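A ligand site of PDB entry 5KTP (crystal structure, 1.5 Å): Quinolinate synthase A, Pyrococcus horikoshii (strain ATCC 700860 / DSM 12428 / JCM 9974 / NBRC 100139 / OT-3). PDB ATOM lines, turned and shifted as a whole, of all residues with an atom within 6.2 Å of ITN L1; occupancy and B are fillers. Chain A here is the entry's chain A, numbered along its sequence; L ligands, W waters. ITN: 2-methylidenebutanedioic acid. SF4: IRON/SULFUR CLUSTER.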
ATOM      1  N   HIS A  25      37.894 -15.520  25.067  1.00  0.00           N
ATOM      2  CA  HIS A  25      36.712 -14.998  24.418  1.00  0.00           C
ATOM      3  C   HIS A  25      36.494 -13.525  24.808  1.00  0.00           C
ATOM      4  O   HIS A  25      36.944 -13.068  25.866  1.00  0.00           O
ATOM      5  CB  HIS A  25      35.477 -15.825  24.769  1.00  0.00           C
ATOM      6  CG  HIS A  25      34.273 -15.414  23.987  1.00  0.00           C
ATOM      7  ND1 HIS A  25      33.325 -14.556  24.480  1.00  0.00           N
ATOM      8  CD2 HIS A  25      33.911 -15.706  22.715  1.00  0.00           C
ATOM      9  CE1 HIS A  25      32.409 -14.343  23.542  1.00  0.00           C
ATOM     10  NE2 HIS A  25      32.739 -15.040  22.470  1.00  0.00           N
ATOM     11  N   ASN A  26      35.797 -12.793  23.922  1.00  0.00           N
ATOM     12  CA  ASN A  26      35.467 -11.382  24.135  1.00  0.00           C
ATOM     13  C   ASN A  26      34.690 -11.098  25.419  1.00  0.00           C
ATOM     14  O   ASN A  26      34.652  -9.936  25.851  1.00  0.00           O
ATOM     15  CB  ASN A  26      34.657 -10.868  22.931  1.00  0.00           C
ATOM     16  CG  ASN A  26      35.489 -10.712  21.694  1.00  0.00           C
ATOM     17  OD1 ASN A  26      36.635 -10.259  21.762  1.00  0.00           O
ATOM     18  ND2 ASN A  26      34.923 -11.076  20.539  1.00  0.00           N
ATOM     19  N   TYR A  27      34.071 -12.100  26.049  1.00  0.00           N
ATOM     20  CA  TYR A  27      33.291 -11.901  27.271  1.00  0.00           C
ATOM     21  C   TYR A  27      34.110 -12.155  28.525  1.00  0.00           C
ATOM     22  O   TYR A  27      33.559 -12.093  29.632  1.00  0.00           O
ATOM     23  CB  TYR A  27      32.065 -12.815  27.319  1.00  0.00           C
ATOM     24  CG  TYR A  27      31.028 -12.638  26.211  1.00  0.00           C
ATOM     25  CD1 TYR A  27      30.976 -11.475  25.458  1.00  0.00           C
ATOM     26  CD2 TYR A  27      30.107 -13.648  25.949  1.00  0.00           C
ATOM     27  CE1 TYR A  27      30.022 -11.328  24.454  1.00  0.00           C
ATOM     28  CE2 TYR A  27      29.160 -13.506  24.949  1.00  0.00           C
ATOM     29  CZ  TYR A  27      29.121 -12.353  24.214  1.00  0.00           C
ATOM     30  OH  TYR A  27      28.196 -12.202  23.208  1.00  0.00           O
ATOM     31  N   GLY A  40      38.929 -13.195  20.806  1.00  0.00           N
ATOM     32  CA  GLY A  40      38.029 -13.184  19.660  1.00  0.00           C
ATOM     33  C   GLY A  40      36.694 -13.835  19.972  1.00  0.00           C
ATOM     34  O   GLY A  40      36.413 -14.211  21.110  1.00  0.00           O
ATOM     35  N   ASP A  41      35.874 -13.971  18.907  1.00  0.00           N
ATOM     36  CA  ASP A  41      34.555 -14.583  18.976  1.00  0.00           C
ATOM     37  C   ASP A  41      34.694 -16.068  18.669  1.00  0.00           C
ATOM     38  O   ASP A  41      35.813 -16.580  18.527  1.00  0.00           O
ATOM     39  CB  ASP A  41      33.553 -13.856  18.054  1.00  0.00           C
ATOM     40  CG  ASP A  41      33.757 -14.120  16.552  1.00  0.00           C
ATOM     41  OD1 ASP A  41      34.751 -14.754  16.148  1.00  0.00           O
ATOM     42  OD2 ASP A  41      32.886 -13.659  15.755  1.00  0.00           O
ATOM     43  N   SER A  42      33.563 -16.781  18.555  1.00  0.00           N
ATOM     44  CA  SER A  42      33.616 -18.230  18.408  1.00  0.00           C
ATOM     45  C   SER A  42      34.321 -18.629  17.116  1.00  0.00           C
ATOM     46  O   SER A  42      35.158 -19.547  17.112  1.00  0.00           O
ATOM     47  CB  SER A  42      32.207 -18.825  18.471  1.00  0.00           C
ATOM     48  OG  SER A  42      31.690 -18.860  19.814  1.00  0.00           O
ATOM     49  N   LEU A  43      34.029 -17.921  16.010  1.00  0.00           N
ATOM     50  CA  LEU A  43      34.587 -18.277  14.709  1.00  0.00           C
ATOM     51  C   LEU A  43      36.080 -17.957  14.632  1.00  0.00           C
ATOM     52  O   LEU A  43      36.850 -18.753  14.076  1.00  0.00           O
ATOM     53  CB  LEU A  43      33.814 -17.550  13.594  1.00  0.00           C
ATOM     54  CG  LEU A  43      34.304 -17.834  12.166  1.00  0.00           C
ATOM     55  CD1 LEU A  43      34.342 -19.330  11.858  1.00  0.00           C
ATOM     56  CD2 LEU A  43      33.432 -17.121  11.147  1.00  0.00           C
ATOM     57  N   PHE A  64      32.420 -25.632  25.619  1.00  0.00           N
ATOM     58  CA  PHE A  64      32.280 -25.994  24.207  1.00  0.00           C
ATOM     59  C   PHE A  64      33.356 -25.329  23.353  1.00  0.00           C
ATOM     60  O   PHE A  64      33.731 -25.871  22.305  1.00  0.00           O
ATOM     61  CB  PHE A  64      30.860 -25.672  23.678  1.00  0.00           C
ATOM     62  CG  PHE A  64      30.586 -24.204  23.371  1.00  0.00           C
ATOM     63  CD1 PHE A  64      31.026 -23.606  22.188  1.00  0.00           C
ATOM     64  CD2 PHE A  64      29.815 -23.446  24.239  1.00  0.00           C
ATOM     65  CE1 PHE A  64      30.753 -22.271  21.920  1.00  0.00           C
ATOM     66  CE2 PHE A  64      29.534 -22.105  23.968  1.00  0.00           C
ATOM     67  CZ  PHE A  64      30.006 -21.519  22.817  1.00  0.00           C
ATOM     68  N   MET A  65      33.859 -24.180  23.790  1.00  0.00           N
ATOM     69  CA  MET A  65      34.905 -23.500  23.045  1.00  0.00           C
ATOM     70  C   MET A  65      36.233 -24.217  23.191  1.00  0.00           C
ATOM     71  O   MET A  65      36.957 -24.405  22.208  1.00  0.00           O
ATOM     72  CB  MET A  65      35.031 -22.058  23.509  1.00  0.00           C
ATOM     73  CG  MET A  65      33.768 -21.240  23.358  1.00  0.00           C
ATOM     74  SD  MET A  65      33.939 -19.532  23.960  1.00  0.00           S
ATOM     75  CE  MET A  65      32.324 -18.916  23.464  1.00  0.00           C
ATOM     76  N   MET A  89      23.023 -22.263  26.943  1.00  0.00           N
ATOM     77  CA  MET A  89      22.341 -22.491  25.675  1.00  0.00           C
ATOM     78  C   MET A  89      22.806 -23.785  25.023  1.00  0.00           C
ATOM     79  O   MET A  89      21.983 -24.599  24.585  1.00  0.00           O
ATOM     80  CB  MET A  89      22.543 -21.292  24.739  1.00  0.00           C
ATOM     81  CG  MET A  89      21.762 -21.401  23.416  1.00  0.00           C
ATOM     82  SD  MET A  89      22.880 -21.727  22.046  1.00  0.00           S
ATOM     83  CE  MET A  89      23.691 -20.133  21.970  1.00  0.00           C
ATOM     84  N   TYR A 113      25.103 -24.748  15.511  1.00  0.00           N
ATOM     85  CA  TYR A 113      25.864 -23.671  16.125  1.00  0.00           C
ATOM     86  C   TYR A 113      27.087 -24.258  16.813  1.00  0.00           C
ATOM     87  O   TYR A 113      27.017 -25.346  17.414  1.00  0.00           O
ATOM     88  CB  TYR A 113      24.973 -22.957  17.151  1.00  0.00           C
ATOM     89  CG  TYR A 113      25.163 -21.466  17.402  1.00  0.00           C
ATOM     90  CD1 TYR A 113      26.039 -20.689  16.645  1.00  0.00           C
ATOM     91  CD2 TYR A 113      24.438 -20.842  18.399  1.00  0.00           C
ATOM     92  CE1 TYR A 113      26.180 -19.321  16.915  1.00  0.00           C
ATOM     93  CE2 TYR A 113      24.563 -19.516  18.662  1.00  0.00           C
ATOM     94  CZ  TYR A 113      25.436 -18.752  17.923  1.00  0.00           C
ATOM     95  OH  TYR A 113      25.523 -17.419  18.228  1.00  0.00           O
ATOM     96  N   VAL A 114      28.223 -23.577  16.706  1.00  0.00           N
ATOM     97  CA  VAL A 114      29.389 -24.012  17.472  1.00  0.00           C
ATOM     98  C   VAL A 114      29.084 -24.004  18.965  1.00  0.00           C
ATOM     99  O   VAL A 114      29.761 -24.703  19.728  1.00  0.00           O
ATOM    100  CB  VAL A 114      30.629 -23.140  17.163  1.00  0.00           C
ATOM    101  CG1 VAL A 114      31.106 -23.406  15.735  1.00  0.00           C
ATOM    102  CG2 VAL A 114      30.299 -21.682  17.402  1.00  0.00           C
ATOM    103  N   ASN A 115      28.083 -23.244  19.403  1.00  0.00           N
ATOM    104  CA  ASN A 115      27.607 -23.327  20.781  1.00  0.00           C
ATOM    105  C   ASN A 115      26.872 -24.656  20.949  1.00  0.00           C
ATOM    106  O   ASN A 115      25.641 -24.715  20.999  1.00  0.00           O
ATOM    107  CB  ASN A 115      26.701 -22.144  21.123  1.00  0.00           C
ATOM    108  CG  ASN A 115      27.382 -20.791  20.938  1.00  0.00           C
ATOM    109  OD1 ASN A 115      28.062 -20.555  19.955  1.00  0.00           O
ATOM    110  ND2 ASN A 115      27.190 -19.895  21.907  1.00  0.00           N
ATOM    111  N   VAL A 128      28.291 -23.804  12.461  1.00  0.00           N
ATOM    112  CA  VAL A 128      28.185 -22.387  12.162  1.00  0.00           C
ATOM    113  C   VAL A 128      28.403 -21.591  13.441  1.00  0.00           C
ATOM    114  O   VAL A 128      28.325 -22.113  14.549  1.00  0.00           O
ATOM    115  CB  VAL A 128      26.824 -21.966  11.539  1.00  0.00           C
ATOM    116  CG1 VAL A 128      26.631 -22.555  10.156  1.00  0.00           C
ATOM    117  CG2 VAL A 128      25.659 -22.291  12.479  1.00  0.00           C
ATOM    118  N   THR A 129      28.685 -20.310  13.264  1.00  0.00           N
ATOM    119  CA  THR A 129      28.668 -19.336  14.344  1.00  0.00           C
ATOM    120  C   THR A 129      27.726 -18.217  13.917  1.00  0.00           C
ATOM    121  O   THR A 129      27.231 -18.200  12.789  1.00  0.00           O
ATOM    122  CB  THR A 129      30.063 -18.771  14.641  1.00  0.00           C
ATOM    123  OG1 THR A 129      30.400 -17.802  13.647  1.00  0.00           O
ATOM    124  CG2 THR A 129      31.124 -19.879  14.600  1.00  0.00           C
ATOM    125  N   SER A 130      27.491 -17.256  14.818  1.00  0.00           N
ATOM    126  CA  SER A 130      26.654 -16.124  14.453  1.00  0.00           C
ATOM    127  C   SER A 130      27.250 -15.350  13.281  1.00  0.00           C
ATOM    128  O   SER A 130      26.522 -14.690  12.539  1.00  0.00           O
ATOM    129  CB  SER A 130      26.459 -15.188  15.649  1.00  0.00           C
ATOM    130  OG  SER A 130      25.552 -15.746  16.584  1.00  0.00           O
ATOM    131  N   ALA A 131      28.572 -15.447  13.093  1.00  0.00           N
ATOM    132  CA  ALA A 131      29.245 -14.676  12.063  1.00  0.00           C
ATOM    133  C   ALA A 131      29.029 -15.248  10.671  1.00  0.00           C
ATOM    134  O   ALA A 131      28.983 -14.480   9.695  1.00  0.00           O
ATOM    135  CB  ALA A 131      30.739 -14.596  12.369  1.00  0.00           C
ATOM    136  N   HIS A 200      23.309  -8.390  19.113  1.00  0.00           N
ATOM    137  CA  HIS A 200      23.660  -9.769  18.837  1.00  0.00           C
ATOM    138  C   HIS A 200      22.435 -10.515  18.313  1.00  0.00           C
ATOM    139  O   HIS A 200      21.329 -10.309  18.812  1.00  0.00           O
ATOM    140  CB  HIS A 200      24.207 -10.439  20.109  1.00  0.00           C
ATOM    141  CG  HIS A 200      25.052 -11.648  19.843  1.00  0.00           C
ATOM    142  ND1 HIS A 200      24.516 -12.881  19.501  1.00  0.00           N
ATOM    143  CD2 HIS A 200      26.397 -11.827  19.879  1.00  0.00           C
ATOM    144  CE1 HIS A 200      25.489 -13.749  19.342  1.00  0.00           C
ATOM    145  NE2 HIS A 200      26.636 -13.140  19.551  1.00  0.00           N
ATOM    146  N   GLU A 202      21.558 -13.377  19.034  1.00  0.00           N
ATOM    147  CA  GLU A 202      20.937 -14.169  20.094  1.00  0.00           C
ATOM    148  C   GLU A 202      19.858 -13.382  20.860  1.00  0.00           C
ATOM    149  O   GLU A 202      19.148 -13.979  21.679  1.00  0.00           O
ATOM    150  CB  GLU A 202      22.009 -14.692  21.070  1.00  0.00           C
ATOM    151  CG  GLU A 202      22.862 -15.778  20.436  1.00  0.00           C
ATOM    152  CD  GLU A 202      24.018 -16.223  21.313  1.00  0.00           C
ATOM    153  OE1 GLU A 202      24.057 -15.844  22.503  1.00  0.00           O
ATOM    154  OE2 GLU A 202      24.883 -16.953  20.811  1.00  0.00           O
ATOM    155  N   ALA A 215      25.066  -8.519  14.549  1.00  0.00           N
ATOM    156  CA  ALA A 215      26.394  -9.092  14.358  1.00  0.00           C
ATOM    157  C   ALA A 215      26.817  -9.905  15.566  1.00  0.00           C
ATOM    158  O   ALA A 215      26.395  -9.626  16.697  1.00  0.00           O
ATOM    159  CB  ALA A 215      27.418  -7.983  14.091  1.00  0.00           C
ATOM    160  N   SER A 216      27.656 -10.910  15.310  1.00  0.00           N
ATOM    161  CA  SER A 216      28.429 -11.560  16.369  1.00  0.00           C
ATOM    162  C   SER A 216      29.382 -10.545  16.976  1.00  0.00           C
ATOM    163  O   SER A 216      29.589  -9.452  16.444  1.00  0.00           O
ATOM    164  CB  SER A 216      29.222 -12.746  15.799  1.00  0.00           C
ATOM    165  OG  SER A 216      30.361 -12.290  15.089  1.00  0.00           O
ATOM    166  N   THR A 217      30.005 -10.907  18.114  1.00  0.00           N
ATOM    167  CA  THR A 217      30.989  -9.993  18.678  1.00  0.00           C
ATOM    168  C   THR A 217      32.111  -9.710  17.695  1.00  0.00           C
ATOM    169  O   THR A 217      32.619  -8.589  17.637  1.00  0.00           O
ATOM    170  CB  THR A 217      31.558 -10.522  20.002  1.00  0.00           C
ATOM    171  OG1 THR A 217      32.217 -11.778  19.785  1.00  0.00           O
ATOM    172  CG2 THR A 217      30.474 -10.676  21.042  1.00  0.00           C
ATOM    173  N   GLY A 218      32.489 -10.687  16.870  1.00  0.00           N
ATOM    174  CA  GLY A 218      33.508 -10.433  15.859  1.00  0.00           C
ATOM    175  C   GLY A 218      33.030  -9.437  14.819  1.00  0.00           C
ATOM    176  O   GLY A 218      33.761  -8.541  14.413  1.00  0.00           O
ATOM    177  N   THR A 234      24.940  -6.915  23.987  1.00  0.00           N
ATOM    178  CA  THR A 234      25.481  -8.256  24.227  1.00  0.00           C
ATOM    179  C   THR A 234      26.049  -8.261  25.640  1.00  0.00           C
ATOM    180  O   THR A 234      25.860  -7.303  26.410  1.00  0.00           O
ATOM    181  CB  THR A 234      26.486  -8.659  23.141  1.00  0.00           C
ATOM    182  OG1 THR A 234      26.788 -10.066  23.255  1.00  0.00           O
ATOM    183  CG2 THR A 234      27.767  -7.869  23.222  1.00  0.00           C
HETATM  184  C1  ITN L   1      30.057 -14.211  20.075  1.00  0.00           C
HETATM  185  C2  ITN L   1      29.530 -15.488  20.670  1.00  0.00           C
HETATM  186  C3  ITN L   1      28.950 -16.375  19.609  1.00  0.00           C
HETATM  187  C5  ITN L   1      29.525 -16.478  18.251  1.00  0.00           C
HETATM  188  O3  ITN L   1      28.929 -17.127  17.403  1.00  0.00           O
HETATM  189  O4  ITN L   1      30.583 -15.922  17.960  1.00  0.00           O
HETATM  190  C4  ITN L   1      27.876 -17.087  19.942  1.00  0.00           C
HETATM  191  O1  ITN L   1      31.175 -13.858  20.399  1.00  0.00           O
HETATM  192  O2  ITN L   1      29.375 -13.563  19.293  1.00  0.00           O
HETATM  193 FE1  SF4 L   2      26.333 -19.449  26.355  1.00  0.00          FE
HETATM  194 FE2  SF4 L   2      27.120 -17.524  28.029  1.00  0.00          FE
HETATM  195 FE3  SF4 L   2      24.973 -17.160  26.411  1.00  0.00          FE
HETATM  196 FE4  SF4 L   2      27.412 -17.306  25.349  1.00  0.00          FE
HETATM  197  S1  SF4 L   2      26.615 -15.718  26.783  1.00  0.00           S
HETATM  198  S2  SF4 L   2      25.510 -18.330  24.597  1.00  0.00           S
HETATM  199  S3  SF4 L   2      28.438 -18.742  26.763  1.00  0.00           S
HETATM  200  S4  SF4 L   2      25.130 -18.688  28.101  1.00  0.00           S
HETATM  201  O   HOH W   1      27.264 -15.419  22.865  1.00  0.00           O
HETATM  202  O   HOH W   2      29.061 -16.989  23.734  1.00  0.00           O
HETATM  203  O   HOH W   3      31.582 -16.086  15.699  1.00  0.00           O
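ND2 of Asn 115 sits close to S2 of SF4 L2, 3.5 Å away. O1 of ITN L1 lies within hydrogen-bond range of NE2 of His 25 (2.9 Å). An oxygen (O1) of ITN L1 sits at hydrogen-bond distance from the side-chain hydroxyl (OG1) of Thr 217 (2.4 Å). The backbone NH (N) of Ser 130 lies within hydrogen-bond range of an oxygen (O3) of ITN L1 (3.0 Å). O2 of ITN L1 lies within hydrogen-bond range of N of Thr 217. An oxygen (O4) of ITN L1 lies within hydrogen-bond range of the backbone NH (N) of Ser 42, at 3.2 Å. An oxygen (O2) of ITN L1 lies within hydrogen-bond range of a ring nitrogen (NE2) of His 200, at 2.8 Å.
OD1 of Asp 41 lies within hydrogen-bond range of N of Leu 43. ND1 of His 200 is in hydrogen-bond range of N of Glu 202, at 3.0 Å. The backbone NH (N) of Ala 131 sits close to the side-chain hydroxyl (OG1) of Thr 129 (3.0 Å). OD2 of Asp 41 lies within hydrogen-bond range of N of Gly 218 (3.2 Å). N of Tyr 27 is in hydrogen-bond range of ND1 of His 25 (3.0 Å). The side-chain hydroxyl (OG1) of Thr 217 sits at hydrogen-bond distance from the side-chain amide nitrogen (ND2) of Asn 26, 2.9 Å away. The side-chain amide nitrogen of Asn 26 lies close to the backbone NH of Asp 41, 3.5 Å away. The backbone NH (N) of Gly 218 sits close to the side-chain hydroxyl (OG) of Ser 216.
Merely in contact with ITN L1: Tyr 113, Glu 202, Asp 41, Thr 129, Asn 115 and Ser 216. Hydrophobic or aromatic side chains that line ITN L1: His 25, Tyr 113 and His 200. Of the 24 residues printed, 11 come within 4 Å of ITN L1. The nearest printed residue that does not touch ITN L1 is Tyr 27 (4.2 Å).
Water W3 lies within hydrogen-bond range of an oxygen (O4) of ITN L1, the side-chain carboxylate (OD2) of Asp 41, the side-chain hydroxyl (OG1) of Thr 129 and the backbone NH (N) of Leu 43. Water W1 bridges the side-chain carboxylate of Glu 202 (3.3 Å) and the side-chain hydroxyl of Tyr 27 (3.4 Å).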
